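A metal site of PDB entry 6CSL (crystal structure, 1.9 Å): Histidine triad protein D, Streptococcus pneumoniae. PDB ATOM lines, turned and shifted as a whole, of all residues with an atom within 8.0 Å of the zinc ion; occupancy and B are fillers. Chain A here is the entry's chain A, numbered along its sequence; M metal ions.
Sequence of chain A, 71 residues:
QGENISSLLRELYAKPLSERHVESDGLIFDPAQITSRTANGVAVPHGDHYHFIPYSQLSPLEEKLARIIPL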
ATOM      1  N   GLU A  23      19.446  19.273  -2.020  1.00  0.00           N
ATOM      2  CA  GLU A  23      18.958  20.512  -1.435  1.00  0.00           C
ATOM      3  C   GLU A  23      19.008  21.630  -2.470  1.00  0.00           C
ATOM      4  O   GLU A  23      19.648  21.519  -3.527  1.00  0.00           O
ATOM      5  CB  GLU A  23      19.783  20.877  -0.205  1.00  0.00           C
ATOM      6  CG  GLU A  23      19.570  19.922   0.970  1.00  0.00           C
ATOM      7  CD  GLU A  23      18.339  20.260   1.784  1.00  0.00           C
ATOM      8  OE1 GLU A  23      18.382  21.277   2.519  1.00  0.00           O
ATOM      9  OE2 GLU A  23      17.332  19.533   1.688  1.00  0.00           O
ATOM     10  N   SER A  24      18.311  22.733  -2.173  1.00  0.00           N
ATOM     11  CA  SER A  24      18.173  23.815  -3.138  1.00  0.00           C
ATOM     12  C   SER A  24      19.527  24.406  -3.533  1.00  0.00           C
ATOM     13  O   SER A  24      19.664  24.924  -4.639  1.00  0.00           O
ATOM     14  CB  SER A  24      17.253  24.906  -2.594  1.00  0.00           C
ATOM     15  OG  SER A  24      17.767  25.445  -1.378  1.00  0.00           O
ATOM     16  N   ASP A  25      20.518  24.339  -2.637  1.00  0.00           N
ATOM     17  CA  ASP A  25      21.835  24.877  -2.928  1.00  0.00           C
ATOM     18  C   ASP A  25      22.803  23.825  -3.439  1.00  0.00           C
ATOM     19  O   ASP A  25      24.010  24.073  -3.520  1.00  0.00           O
ATOM     20  CB  ASP A  25      22.413  25.581  -1.681  1.00  0.00           C
ATOM     21  CG  ASP A  25      22.908  24.618  -0.617  1.00  0.00           C
ATOM     22  OD1 ASP A  25      22.711  23.395  -0.726  1.00  0.00           O
ATOM     23  OD2 ASP A  25      23.513  25.112   0.359  1.00  0.00           O
ATOM     24  N   GLY A  26      22.298  22.630  -3.792  1.00  0.00           N
ATOM     25  CA  GLY A  26      23.107  21.621  -4.450  1.00  0.00           C
ATOM     26  C   GLY A  26      23.577  20.488  -3.563  1.00  0.00           C
ATOM     27  O   GLY A  26      24.038  19.476  -4.098  1.00  0.00           O
ATOM     28  N   LEU A  27      23.474  20.631  -2.248  1.00  0.00           N
ATOM     29  CA  LEU A  27      23.960  19.590  -1.352  1.00  0.00           C
ATOM     30  C   LEU A  27      23.210  18.288  -1.577  1.00  0.00           C
ATOM     31  O   LEU A  27      21.976  18.253  -1.522  1.00  0.00           O
ATOM     32  CB  LEU A  27      23.832  20.030   0.108  1.00  0.00           C
ATOM     33  CG  LEU A  27      24.280  18.980   1.143  1.00  0.00           C
ATOM     34  CD1 LEU A  27      25.794  18.787   1.077  1.00  0.00           C
ATOM     35  CD2 LEU A  27      23.859  19.368   2.548  1.00  0.00           C
ATOM     36  N   ILE A  28      23.957  17.218  -1.820  1.00  0.00           N
ATOM     37  CA  ILE A  28      23.407  15.868  -1.890  1.00  0.00           C
ATOM     38  C   ILE A  28      23.400  15.275  -0.489  1.00  0.00           C
ATOM     39  O   ILE A  28      24.432  15.283   0.193  1.00  0.00           O
ATOM     40  CB  ILE A  28      24.220  14.996  -2.857  1.00  0.00           C
ATOM     41  CG1 ILE A  28      24.149  15.548  -4.289  1.00  0.00           C
ATOM     42  CG2 ILE A  28      23.743  13.540  -2.817  1.00  0.00           C
ATOM     43  CD1 ILE A  28      22.771  15.504  -4.911  1.00  0.00           C
ATOM     44  N   VAL A  44      22.965  17.889   8.536  1.00  0.00           N
ATOM     45  CA  VAL A  44      24.190  17.588   7.801  1.00  0.00           C
ATOM     46  C   VAL A  44      24.977  18.884   7.591  1.00  0.00           C
ATOM     47  O   VAL A  44      24.373  19.925   7.296  1.00  0.00           O
ATOM     48  CB  VAL A  44      23.893  16.910   6.453  1.00  0.00           C
ATOM     49  CG1 VAL A  44      23.421  15.473   6.679  1.00  0.00           C
ATOM     50  CG2 VAL A  44      22.855  17.698   5.670  1.00  0.00           C
ATOM     51  N   PRO A  45      26.300  18.870   7.734  1.00  0.00           N
ATOM     52  CA  PRO A  45      27.083  20.086   7.526  1.00  0.00           C
ATOM     53  C   PRO A  45      27.297  20.381   6.050  1.00  0.00           C
ATOM     54  O   PRO A  45      27.324  19.491   5.200  1.00  0.00           O
ATOM     55  CB  PRO A  45      28.410  19.765   8.214  1.00  0.00           C
ATOM     56  CG  PRO A  45      28.547  18.291   8.068  1.00  0.00           C
ATOM     57  CD  PRO A  45      27.142  17.733   8.147  1.00  0.00           C
ATOM     58  N   HIS A  46      27.475  21.679   5.755  1.00  0.00           N
ATOM     59  CA  HIS A  46      27.742  22.115   4.379  1.00  0.00           C
ATOM     60  C   HIS A  46      28.542  23.417   4.478  1.00  0.00           C
ATOM     61  O   HIS A  46      28.036  24.513   4.268  1.00  0.00           O
ATOM     62  CB  HIS A  46      26.464  22.309   3.568  1.00  0.00           C
ATOM     63  CG  HIS A  46      26.700  22.503   2.099  1.00  0.00           C
ATOM     64  ND1 HIS A  46      25.864  23.240   1.301  1.00  0.00           N
ATOM     65  CD2 HIS A  46      27.680  22.040   1.292  1.00  0.00           C
ATOM     66  CE1 HIS A  46      26.317  23.236   0.059  1.00  0.00           C
ATOM     67  NE2 HIS A  46      27.418  22.511   0.025  1.00  0.00           N
ATOM     68  N   GLY A  47      29.821  23.271   4.817  1.00  0.00           N
ATOM     69  CA  GLY A  47      30.692  24.425   4.940  1.00  0.00           C
ATOM     70  C   GLY A  47      30.366  25.284   6.141  1.00  0.00           C
ATOM     71  O   GLY A  47      30.394  24.810   7.281  1.00  0.00           O
ATOM     72  N   ASP A  48      30.027  26.549   5.894  1.00  0.00           N
ATOM     73  CA  ASP A  48      29.746  27.497   6.969  1.00  0.00           C
ATOM     74  C   ASP A  48      28.312  27.403   7.476  1.00  0.00           C
ATOM     75  O   ASP A  48      27.869  28.318   8.175  1.00  0.00           O
ATOM     76  CB  ASP A  48      30.049  28.923   6.513  1.00  0.00           C
ATOM     77  CG  ASP A  48      29.210  29.361   5.326  1.00  0.00           C
ATOM     78  OD1 ASP A  48      28.184  28.716   5.026  1.00  0.00           O
ATOM     79  OD2 ASP A  48      29.575  30.377   4.689  1.00  0.00           O
ATOM     80  N   HIS A  49      27.585  26.342   7.144  1.00  0.00           N
ATOM     81  CA  HIS A  49      26.217  26.185   7.610  1.00  0.00           C
ATOM     82  C   HIS A  49      25.869  24.704   7.645  1.00  0.00           C
ATOM     83  O   HIS A  49      26.533  23.877   7.018  1.00  0.00           O
ATOM     84  CB  HIS A  49      25.220  26.939   6.722  1.00  0.00           C
ATOM     85  CG  HIS A  49      25.214  26.477   5.295  1.00  0.00           C
ATOM     86  ND1 HIS A  49      26.164  26.878   4.378  1.00  0.00           N
ATOM     87  CD2 HIS A  49      24.390  25.636   4.634  1.00  0.00           C
ATOM     88  CE1 HIS A  49      25.911  26.308   3.220  1.00  0.00           C
ATOM     89  NE2 HIS A  49      24.837  25.553   3.342  1.00  0.00           N
ATOM     90  N   TYR A  50      24.820  24.386   8.399  1.00  0.00           N
ATOM     91  CA  TYR A  50      24.239  23.046   8.444  1.00  0.00           C
ATOM     92  C   TYR A  50      22.850  23.086   7.818  1.00  0.00           C
ATOM     93  O   TYR A  50      22.108  24.055   7.984  1.00  0.00           O
ATOM     94  CB  TYR A  50      24.110  22.522   9.874  1.00  0.00           C
ATOM     95  CG  TYR A  50      25.397  22.399  10.650  1.00  0.00           C
ATOM     96  CD1 TYR A  50      25.998  23.513  11.219  1.00  0.00           C
ATOM     97  CD2 TYR A  50      25.992  21.160  10.842  1.00  0.00           C
ATOM     98  CE1 TYR A  50      27.168  23.394  11.936  1.00  0.00           C
ATOM     99  CE2 TYR A  50      27.169  21.035  11.557  1.00  0.00           C
ATOM    100  CZ  TYR A  50      27.752  22.152  12.109  1.00  0.00           C
ATOM    101  OH  TYR A  50      28.908  22.046  12.831  1.00  0.00           O
ATOM    102  N   HIS A  51      22.500  22.008   7.122  1.00  0.00           N
ATOM    103  CA  HIS A  51      21.135  21.784   6.704  1.00  0.00           C
ATOM    104  C   HIS A  51      20.431  20.908   7.734  1.00  0.00           C
ATOM    105  O   HIS A  51      21.055  20.051   8.373  1.00  0.00           O
ATOM    106  CB  HIS A  51      21.072  21.093   5.342  1.00  0.00           C
ATOM    107  CG  HIS A  51      21.622  21.903   4.214  1.00  0.00           C
ATOM    108  ND1 HIS A  51      20.864  22.292   3.131  1.00  0.00           N
ATOM    109  CD2 HIS A  51      22.860  22.400   3.996  1.00  0.00           C
ATOM    110  CE1 HIS A  51      21.608  22.991   2.289  1.00  0.00           C
ATOM    111  NE2 HIS A  51      22.835  23.075   2.790  1.00  0.00           N
HETATM  112 ZN    ZN M   1      24.263  24.200   1.920  1.00  0.00          ZN
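Four residues have an atom within 4 Å of the zinc ion: Asp 25, His 46, His 49 and His 51. The nearest printed residue that does not touch the zinc ion is Leu 27 (4.6 Å).
OD2 of Asp 25 is bound to the zinc ion, at 2.0 Å. ND1 of His 46 binds the zinc ion (2.0 Å). The zinc ion is bound by a ring nitrogen (NE2) of His 51 (2.0 Å). A ring nitrogen (NE2) of His 49 is bound to the zinc ion (2.0 Å).
A ring nitrogen (ND1) of His 49 sits at hydrogen-bond distance from the side-chain carboxylate of Asp 48 (2.8 Å). The side-chain carboxylate of Asp 25 lies within hydrogen-bond range of the backbone NH of Leu 27 (3.2 Å). The side-chain carboxylate (OE1) of Glu 23 sits at hydrogen-bond distance from a ring nitrogen (ND1) of His 51, 2.8 Å away. O of Val 44 sits at hydrogen-bond distance from N of His 51, at 2.8 Å.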
